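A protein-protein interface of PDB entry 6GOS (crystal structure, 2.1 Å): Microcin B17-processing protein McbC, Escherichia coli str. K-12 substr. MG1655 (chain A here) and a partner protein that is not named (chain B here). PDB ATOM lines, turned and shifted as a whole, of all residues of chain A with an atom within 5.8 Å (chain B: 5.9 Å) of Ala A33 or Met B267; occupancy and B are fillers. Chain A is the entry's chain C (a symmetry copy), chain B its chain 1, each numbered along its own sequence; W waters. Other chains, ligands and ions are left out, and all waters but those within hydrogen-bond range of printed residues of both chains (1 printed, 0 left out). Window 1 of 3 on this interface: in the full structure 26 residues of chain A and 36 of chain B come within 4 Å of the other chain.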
ATOM      1  N   ASN A  31     -13.677 -11.577  20.547  1.00  0.00           N
ATOM      2  CA  ASN A  31     -13.581 -11.928  19.136  1.00  0.00           C
ATOM      3  C   ASN A  31     -14.711 -11.248  18.371  1.00  0.00           C
ATOM      4  O   ASN A  31     -15.809 -11.070  18.909  1.00  0.00           O
ATOM      5  CB  ASN A  31     -13.694 -13.449  18.946  1.00  0.00           C
ATOM      6  CG  ASN A  31     -12.412 -14.197  19.313  1.00  0.00           C
ATOM      7  OD1 ASN A  31     -11.374 -13.612  19.678  1.00  0.00           O
ATOM      8  ND2 ASN A  31     -12.477 -15.496  19.192  1.00  0.00           N
ATOM      9  N   PHE A  32     -14.431 -10.893  17.121  1.00  0.00           N
ATOM     10  CA  PHE A  32     -15.404 -10.269  16.231  1.00  0.00           C
ATOM     11  C   PHE A  32     -15.868 -11.185  15.110  1.00  0.00           C
ATOM     12  O   PHE A  32     -15.120 -12.042  14.664  1.00  0.00           O
ATOM     13  CB  PHE A  32     -14.784  -9.030  15.586  1.00  0.00           C
ATOM     14  CG  PHE A  32     -14.855  -7.781  16.412  1.00  0.00           C
ATOM     15  CD1 PHE A  32     -15.301  -7.774  17.744  1.00  0.00           C
ATOM     16  CD2 PHE A  32     -14.451  -6.582  15.841  1.00  0.00           C
ATOM     17  CE1 PHE A  32     -15.339  -6.595  18.460  1.00  0.00           C
ATOM     18  CE2 PHE A  32     -14.485  -5.403  16.560  1.00  0.00           C
ATOM     19  CZ  PHE A  32     -14.935  -5.406  17.866  1.00  0.00           C
ATOM     20  N   ALA A  33     -17.110 -10.980  14.681  1.00  0.00           N
ATOM     21  CA  ALA A  33     -17.615 -11.451  13.400  1.00  0.00           C
ATOM     22  C   ALA A  33     -17.759 -10.224  12.494  1.00  0.00           C
ATOM     23  O   ALA A  33     -18.791  -9.560  12.473  1.00  0.00           O
ATOM     24  CB  ALA A  33     -18.951 -12.157  13.560  1.00  0.00           C
ATOM     25  N   SER A  34     -16.689  -9.946  11.754  1.00  0.00           N
ATOM     26  CA  SER A  34     -16.536  -8.760  10.961  1.00  0.00           C
ATOM     27  C   SER A  34     -16.352  -9.183   9.499  1.00  0.00           C
ATOM     28  O   SER A  34     -15.265  -9.565   9.080  1.00  0.00           O
ATOM     29  CB  SER A  34     -15.316  -8.013  11.474  1.00  0.00           C
ATOM     30  OG  SER A  34     -15.027  -6.887  10.672  1.00  0.00           O
ATOM     31  N   LEU A  35     -17.424  -9.129   8.727  1.00  0.00           N
ATOM     32  CA  LEU A  35     -17.417  -9.568   7.322  1.00  0.00           C
ATOM     33  C   LEU A  35     -18.218  -8.582   6.500  1.00  0.00           C
ATOM     34  O   LEU A  35     -19.202  -8.086   7.002  1.00  0.00           O
ATOM     35  CB  LEU A  35     -18.113 -10.928   7.202  1.00  0.00           C
ATOM     36  CG  LEU A  35     -17.429 -12.195   7.712  1.00  0.00           C
ATOM     37  CD1 LEU A  35     -18.335 -13.402   7.514  1.00  0.00           C
ATOM     38  CD2 LEU A  35     -16.093 -12.407   7.002  1.00  0.00           C
ATOM     39  N   PHE A  38     -21.899  -9.127   6.662  1.00  0.00           N
ATOM     40  CA  PHE A  38     -22.636  -8.836   7.895  1.00  0.00           C
ATOM     41  C   PHE A  38     -22.807  -7.320   8.171  1.00  0.00           C
ATOM     42  O   PHE A  38     -23.309  -6.944   9.226  1.00  0.00           O
ATOM     43  CB  PHE A  38     -21.969  -9.500   9.098  1.00  0.00           C
ATOM     44  CG  PHE A  38     -21.832 -11.005   9.029  1.00  0.00           C
ATOM     45  CD1 PHE A  38     -22.631 -11.803   8.222  1.00  0.00           C
ATOM     46  CD2 PHE A  38     -20.901 -11.628   9.869  1.00  0.00           C
ATOM     47  CE1 PHE A  38     -22.480 -13.177   8.220  1.00  0.00           C
ATOM     48  CE2 PHE A  38     -20.742 -13.010   9.868  1.00  0.00           C
ATOM     49  CZ  PHE A  38     -21.539 -13.789   9.038  1.00  0.00           C
ATOM     50  N   THR A  42     -25.045  -5.736  11.589  1.00  0.00           N
ATOM     51  CA  THR A  42     -24.210  -5.668  12.778  1.00  0.00           C
ATOM     52  C   THR A  42     -23.686  -4.250  12.983  1.00  0.00           C
ATOM     53  O   THR A  42     -23.844  -3.380  12.109  1.00  0.00           O
ATOM     54  CB  THR A  42     -23.012  -6.624  12.690  1.00  0.00           C
ATOM     55  OG1 THR A  42     -22.171  -6.257  11.594  1.00  0.00           O
ATOM     56  CG2 THR A  42     -23.482  -8.055  12.552  1.00  0.00           C
ATOM     57  N   TYR A 238     -11.226  -7.503  12.269  1.00  0.00           N
ATOM     58  CA  TYR A 238     -11.153  -8.774  11.577  1.00  0.00           C
ATOM     59  C   TYR A 238     -11.886  -9.844  12.365  1.00  0.00           C
ATOM     60  O   TYR A 238     -12.060  -9.745  13.577  1.00  0.00           O
ATOM     61  CB  TYR A 238      -9.684  -9.158  11.322  1.00  0.00           C
ATOM     62  CG  TYR A 238      -8.902  -9.375  12.589  1.00  0.00           C
ATOM     63  CD1 TYR A 238      -8.927 -10.594  13.239  1.00  0.00           C
ATOM     64  CD2 TYR A 238      -8.168  -8.346  13.165  1.00  0.00           C
ATOM     65  CE1 TYR A 238      -8.222 -10.795  14.413  1.00  0.00           C
ATOM     66  CE2 TYR A 238      -7.462  -8.539  14.344  1.00  0.00           C
ATOM     67  CZ  TYR A 238      -7.495  -9.762  14.962  1.00  0.00           C
ATOM     68  OH  TYR A 238      -6.809  -9.976  16.144  1.00  0.00           O
ATOM     69  N   THR A 239     -12.314 -10.868  11.647  1.00  0.00           N
ATOM     70  CA  THR A 239     -12.918 -12.030  12.243  1.00  0.00           C
ATOM     71  C   THR A 239     -11.805 -12.962  12.740  1.00  0.00           C
ATOM     72  O   THR A 239     -11.140 -13.611  11.950  1.00  0.00           O
ATOM     73  CB  THR A 239     -13.827 -12.732  11.219  1.00  0.00           C
ATOM     74  OG1 THR A 239     -14.795 -11.799  10.728  1.00  0.00           O
ATOM     75  CG2 THR A 239     -14.516 -13.922  11.826  1.00  0.00           C
ATOM     76  N   TRP B  95     -25.148 -16.643   3.340  1.00  0.00           N
ATOM     77  CA  TRP B  95     -25.872 -17.828   2.993  1.00  0.00           C
ATOM     78  C   TRP B  95     -27.022 -17.378   2.122  1.00  0.00           C
ATOM     79  O   TRP B  95     -27.846 -16.554   2.534  1.00  0.00           O
ATOM     80  CB  TRP B  95     -26.323 -18.568   4.269  1.00  0.00           C
ATOM     81  CG  TRP B  95     -25.153 -18.760   5.137  1.00  0.00           C
ATOM     82  CD1 TRP B  95     -24.071 -19.531   4.864  1.00  0.00           C
ATOM     83  CD2 TRP B  95     -24.866 -18.078   6.350  1.00  0.00           C
ATOM     84  NE1 TRP B  95     -23.143 -19.388   5.835  1.00  0.00           N
ATOM     85  CE2 TRP B  95     -23.609 -18.509   6.771  1.00  0.00           C
ATOM     86  CE3 TRP B  95     -25.567 -17.164   7.136  1.00  0.00           C
ATOM     87  CZ2 TRP B  95     -23.033 -18.072   7.960  1.00  0.00           C
ATOM     88  CZ3 TRP B  95     -24.998 -16.712   8.285  1.00  0.00           C
ATOM     89  CH2 TRP B  95     -23.742 -17.166   8.697  1.00  0.00           C
ATOM     90  N   ASP B 181     -27.217 -23.359  19.315  1.00  0.00           N
ATOM     91  CA  ASP B 181     -25.768 -23.239  19.222  1.00  0.00           C
ATOM     92  C   ASP B 181     -25.412 -22.001  18.411  1.00  0.00           C
ATOM     93  O   ASP B 181     -26.186 -21.533  17.607  1.00  0.00           O
ATOM     94  CB  ASP B 181     -25.144 -24.470  18.578  1.00  0.00           C
ATOM     95  CG  ASP B 181     -25.295 -25.718  19.417  1.00  0.00           C
ATOM     96  OD1 ASP B 181     -25.605 -25.614  20.637  1.00  0.00           O
ATOM     97  OD2 ASP B 181     -25.094 -26.820  18.831  1.00  0.00           O
ATOM     98  N   GLY B 182     -24.235 -21.461  18.643  1.00  0.00           N
ATOM     99  CA  GLY B 182     -23.632 -20.566  17.673  1.00  0.00           C
ATOM    100  C   GLY B 182     -23.505 -21.181  16.284  1.00  0.00           C
ATOM    101  O   GLY B 182     -23.664 -22.395  16.080  1.00  0.00           O
ATOM    102  N   VAL B 183     -23.219 -20.318  15.332  1.00  0.00           N
ATOM    103  CA  VAL B 183     -23.146 -20.705  13.959  1.00  0.00           C
ATOM    104  C   VAL B 183     -21.852 -21.466  13.752  1.00  0.00           C
ATOM    105  O   VAL B 183     -20.777 -20.957  14.053  1.00  0.00           O
ATOM    106  CB  VAL B 183     -23.145 -19.488  13.020  1.00  0.00           C
ATOM    107  CG1 VAL B 183     -23.078 -19.959  11.562  1.00  0.00           C
ATOM    108  CG2 VAL B 183     -24.388 -18.648  13.254  1.00  0.00           C
ATOM    109  N   TYR B 184     -21.983 -22.692  13.244  1.00  0.00           N
ATOM    110  CA  TYR B 184     -20.852 -23.527  12.892  1.00  0.00           C
ATOM    111  C   TYR B 184     -20.586 -23.350  11.408  1.00  0.00           C
ATOM    112  O   TYR B 184     -21.383 -23.793  10.573  1.00  0.00           O
ATOM    113  CB  TYR B 184     -21.150 -25.006  13.197  1.00  0.00           C
ATOM    114  CG  TYR B 184     -20.073 -25.958  12.711  1.00  0.00           C
ATOM    115  CD1 TYR B 184     -18.709 -25.622  12.787  1.00  0.00           C
ATOM    116  CD2 TYR B 184     -20.409 -27.180  12.175  1.00  0.00           C
ATOM    117  CE1 TYR B 184     -17.735 -26.481  12.299  1.00  0.00           C
ATOM    118  CE2 TYR B 184     -19.441 -28.052  11.708  1.00  0.00           C
ATOM    119  CZ  TYR B 184     -18.112 -27.703  11.778  1.00  0.00           C
ATOM    120  OH  TYR B 184     -17.177 -28.577  11.303  1.00  0.00           O
ATOM    121  N   SER B 185     -19.483 -22.680  11.089  1.00  0.00           N
ATOM    122  CA  SER B 185     -19.082 -22.409   9.713  1.00  0.00           C
ATOM    123  C   SER B 185     -17.651 -22.865   9.546  1.00  0.00           C
ATOM    124  O   SER B 185     -16.749 -22.202  10.057  1.00  0.00           O
ATOM    125  CB  SER B 185     -19.126 -20.920   9.417  1.00  0.00           C
ATOM    126  OG  SER B 185     -18.320 -20.638   8.263  1.00  0.00           O
ATOM    127  N   LEU B 188     -15.353 -20.157   8.302  1.00  0.00           N
ATOM    128  CA  LEU B 188     -14.987 -19.148   9.310  1.00  0.00           C
ATOM    129  C   LEU B 188     -14.241 -19.679  10.564  1.00  0.00           C
ATOM    130  O   LEU B 188     -13.745 -18.889  11.377  1.00  0.00           O
ATOM    131  CB  LEU B 188     -16.227 -18.369   9.737  1.00  0.00           C
ATOM    132  CG  LEU B 188     -16.916 -17.557   8.629  1.00  0.00           C
ATOM    133  CD1 LEU B 188     -18.258 -17.067   9.120  1.00  0.00           C
ATOM    134  CD2 LEU B 188     -16.081 -16.380   8.145  1.00  0.00           C
ATOM    135  N   THR B 190     -15.492 -21.563  13.174  1.00  0.00           N
ATOM    136  CA  THR B 190     -16.222 -21.401  14.425  1.00  0.00           C
ATOM    137  C   THR B 190     -16.577 -22.746  15.063  1.00  0.00           C
ATOM    138  O   THR B 190     -16.673 -23.750  14.378  1.00  0.00           O
ATOM    139  CB  THR B 190     -17.509 -20.592  14.239  1.00  0.00           C
ATOM    140  OG1 THR B 190     -18.322 -21.215  13.249  1.00  0.00           O
ATOM    141  CG2 THR B 190     -17.186 -19.145  13.795  1.00  0.00           C
ATOM    142  N   ARG B 249     -33.791 -15.530  15.254  1.00  0.00           N
ATOM    143  CA  ARG B 249     -32.370 -15.840  15.053  1.00  0.00           C
ATOM    144  C   ARG B 249     -32.021 -15.936  13.583  1.00  0.00           C
ATOM    145  O   ARG B 249     -31.013 -15.395  13.144  1.00  0.00           O
ATOM    146  CB  ARG B 249     -31.984 -17.141  15.777  1.00  0.00           C
ATOM    147  CG  ARG B 249     -30.486 -17.427  15.704  1.00  0.00           C
ATOM    148  CD  ARG B 249     -29.670 -16.420  16.472  1.00  0.00           C
ATOM    149  NE  ARG B 249     -28.258 -16.726  16.381  1.00  0.00           N
ATOM    150  CZ  ARG B 249     -27.283 -15.897  16.018  1.00  0.00           C
ATOM    151  NH1 ARG B 249     -27.518 -14.621  15.727  1.00  0.00           N
ATOM    152  NH2 ARG B 249     -26.023 -16.357  15.980  1.00  0.00           N
ATOM    153  N   LEU B 253     -29.639 -13.313  11.157  1.00  0.00           N
ATOM    154  CA  LEU B 253     -28.571 -13.806  10.307  1.00  0.00           C
ATOM    155  C   LEU B 253     -28.792 -13.573   8.824  1.00  0.00           C
ATOM    156  O   LEU B 253     -27.845 -13.250   8.101  1.00  0.00           O
ATOM    157  CB  LEU B 253     -28.361 -15.309  10.555  1.00  0.00           C
ATOM    158  CG  LEU B 253     -27.831 -15.662  11.955  1.00  0.00           C
ATOM    159  CD1 LEU B 253     -28.054 -17.129  12.223  1.00  0.00           C
ATOM    160  CD2 LEU B 253     -26.358 -15.353  12.104  1.00  0.00           C
ATOM    161  N   VAL B 263     -20.805  -6.906  16.669  1.00  0.00           N
ATOM    162  CA  VAL B 263     -19.954  -7.896  16.014  1.00  0.00           C
ATOM    163  C   VAL B 263     -19.380  -8.968  16.968  1.00  0.00           C
ATOM    164  O   VAL B 263     -19.065 -10.072  16.521  1.00  0.00           O
ATOM    165  CB  VAL B 263     -18.817  -7.233  15.175  1.00  0.00           C
ATOM    166  CG1 VAL B 263     -19.408  -6.504  13.966  1.00  0.00           C
ATOM    167  CG2 VAL B 263     -17.966  -6.285  16.004  1.00  0.00           C
ATOM    168  N   ASP B 264     -19.279  -8.665  18.269  1.00  0.00           N
ATOM    169  CA  ASP B 264     -18.716  -9.616  19.265  1.00  0.00           C
ATOM    170  C   ASP B 264     -19.631 -10.736  19.795  1.00  0.00           C
ATOM    171  O   ASP B 264     -19.160 -11.588  20.551  1.00  0.00           O
ATOM    172  CB  ASP B 264     -18.054  -8.875  20.445  1.00  0.00           C
ATOM    173  CG  ASP B 264     -19.070  -8.251  21.465  1.00  0.00           C
ATOM    174  OD1 ASP B 264     -20.296  -8.535  21.424  1.00  0.00           O
ATOM    175  OD2 ASP B 264     -18.599  -7.451  22.321  1.00  0.00           O
ATOM    176  N   ASN B 265     -20.917 -10.675  19.440  1.00  0.00           N
ATOM    177  CA  ASN B 265     -21.918 -11.666  19.847  1.00  0.00           C
ATOM    178  C   ASN B 265     -22.770 -12.241  18.713  1.00  0.00           C
ATOM    179  O   ASN B 265     -23.535 -13.176  18.952  1.00  0.00           O
ATOM    180  CB  ASN B 265     -22.842 -11.078  20.938  1.00  0.00           C
ATOM    181  CG  ASN B 265     -23.597  -9.839  20.479  1.00  0.00           C
ATOM    182  OD1 ASN B 265     -24.238  -9.842  19.428  1.00  0.00           O
ATOM    183  ND2 ASN B 265     -23.516  -8.767  21.274  1.00  0.00           N
ATOM    184  N   PHE B 266     -22.592 -11.740  17.484  1.00  0.00           N
ATOM    185  CA  PHE B 266     -23.469 -12.049  16.336  1.00  0.00           C
ATOM    186  C   PHE B 266     -23.583 -13.529  15.956  1.00  0.00           C
ATOM    187  O   PHE B 266     -24.662 -13.998  15.607  1.00  0.00           O
ATOM    188  CB  PHE B 266     -22.969 -11.243  15.131  1.00  0.00           C
ATOM    189  CG  PHE B 266     -23.770 -11.429  13.883  1.00  0.00           C
ATOM    190  CD1 PHE B 266     -25.085 -11.034  13.830  1.00  0.00           C
ATOM    191  CD2 PHE B 266     -23.192 -11.987  12.753  1.00  0.00           C
ATOM    192  CE1 PHE B 266     -25.819 -11.192  12.683  1.00  0.00           C
ATOM    193  CE2 PHE B 266     -23.925 -12.156  11.591  1.00  0.00           C
ATOM    194  CZ  PHE B 266     -25.240 -11.759  11.558  1.00  0.00           C
ATOM    195  N   MET B 267     -22.473 -14.253  16.021  1.00  0.00           N
ATOM    196  CA  MET B 267     -22.451 -15.668  15.680  1.00  0.00           C
ATOM    197  C   MET B 267     -22.622 -16.581  16.897  1.00  0.00           C
ATOM    198  O   MET B 267     -22.569 -17.808  16.752  1.00  0.00           O
ATOM    199  CB  MET B 267     -21.126 -16.006  14.977  1.00  0.00           C
ATOM    200  CG  MET B 267     -20.970 -15.335  13.619  1.00  0.00           C
ATOM    201  SD  MET B 267     -19.522 -15.906  12.704  1.00  0.00           S
ATOM    202  CE  MET B 267     -20.055 -17.571  12.330  1.00  0.00           C
ATOM    203  N   SER B 268     -22.823 -16.008  18.085  1.00  0.00           N
ATOM    204  CA  SER B 268     -22.742 -16.786  19.326  1.00  0.00           C
ATOM    205  C   SER B 268     -24.016 -17.545  19.654  1.00  0.00           C
ATOM    206  O   SER B 268     -25.094 -17.257  19.156  1.00  0.00           O
ATOM    207  CB  SER B 268     -22.375 -15.885  20.510  1.00  0.00           C
ATOM    208  OG  SER B 268     -21.201 -15.156  20.239  1.00  0.00           O
ATOM    209  N   SER B 269     -23.869 -18.496  20.555  1.00  0.00           N
ATOM    210  CA  SER B 269     -24.986 -19.294  21.026  1.00  0.00           C
ATOM    211  C   SER B 269     -26.033 -18.436  21.747  1.00  0.00           C
ATOM    212  O   SER B 269     -25.695 -17.377  22.290  1.00  0.00           O
ATOM    213  CB  SER B 269     -24.465 -20.370  21.998  1.00  0.00           C
ATOM    214  OG  SER B 269     -24.165 -19.803  23.264  1.00  0.00           O
HETATM  215  O   HOH W   1     -17.281 -13.475  20.687  1.00  0.00           O
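O of Val B263 lies within hydrogen-bond range of N of Ala A33 (2.8 Å).
Water W1 lies within hydrogen-bond range of the backbone carbonyl oxygen of Asp B264 and the backbone carbonyl oxygen of Asn A31.
Of the printed residues of chain B, Asn A31 touches Asp B264 (3.3 Å). Of the printed residues of chain B, Phe A32 touches Val B263. Of the printed residues of chain B, Ala A33 touches Val B263 (2.8 Å) and Met B267 (3.8 Å). Val B183 touches none of the printed residues of chain A. Printed residues of chain A within 4 Å of Asp B264: Asn A31 (3.3 Å). Of the printed residues of chain A, Met B267 touches Ala A33 (3.8 Å). Ser B269 touches none of the printed residues of chain A. The nearest printed residue of chain B that does not touch Phe A32 is Asp B264 (4.01 Å).
Printed residues of chain A that touch a printed residue of chain B: Asn A31, Phe A32, Ala A33, Leu A35, Phe A38 and Thr A42. Hydrophobic or aromatic side chains of chain A that line the printed part of chain B: Phe A32, Ala A33, Leu A35 and Phe A38. Of the 17 printed residues of chain B, 5 touch a printed residue of chain A. Hydrophobic or aromatic side chains of chain B within 4 Å of the printed part of chain A: Leu B188, Val B263, Phe B266 and Met B267. Among the printed residues, 8 pairs touch across the chains. Among the printed residues, no Asp or Glu carboxylate lies within 4 Å of a Lys or Arg side-chain nitrogen of the other chain.
O of Asn A31 touches CA of Asp B264, at 3.3 Å. Phe A32 touches Val B263 (CG to CG2, 3.5 Å). Met B267 touches Ala A33. Leu A35 touches Leu B188. CE2 of Phe B266 touches CG of Phe A38, 3.5 Å away. Thr A42 touches Val B263 (OG1 to CG1, 3.6 Å). CD1 of Phe B266 touches CG2 of Thr A42, 3.6 Å away.
N of Val B183 sits at hydrogen-bond distance from O of Met B267, 3.0 Å away. The backbone NH (N) of Leu B188 lies within hydrogen-bond range of the side-chain hydroxyl (OG) of Ser B185, at 3.0 Å. The backbone carbonyl oxygen (O) of Phe B266 is in hydrogen-bond range of the guanidinium group (NH2) of Arg B249 (2.7 Å). OD1 of Asp B264 lies within hydrogen-bond range of ND2 of Asn B265. OG1 of Thr A42 lies within hydrogen-bond range of O of Phe A38 (2.7 Å).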
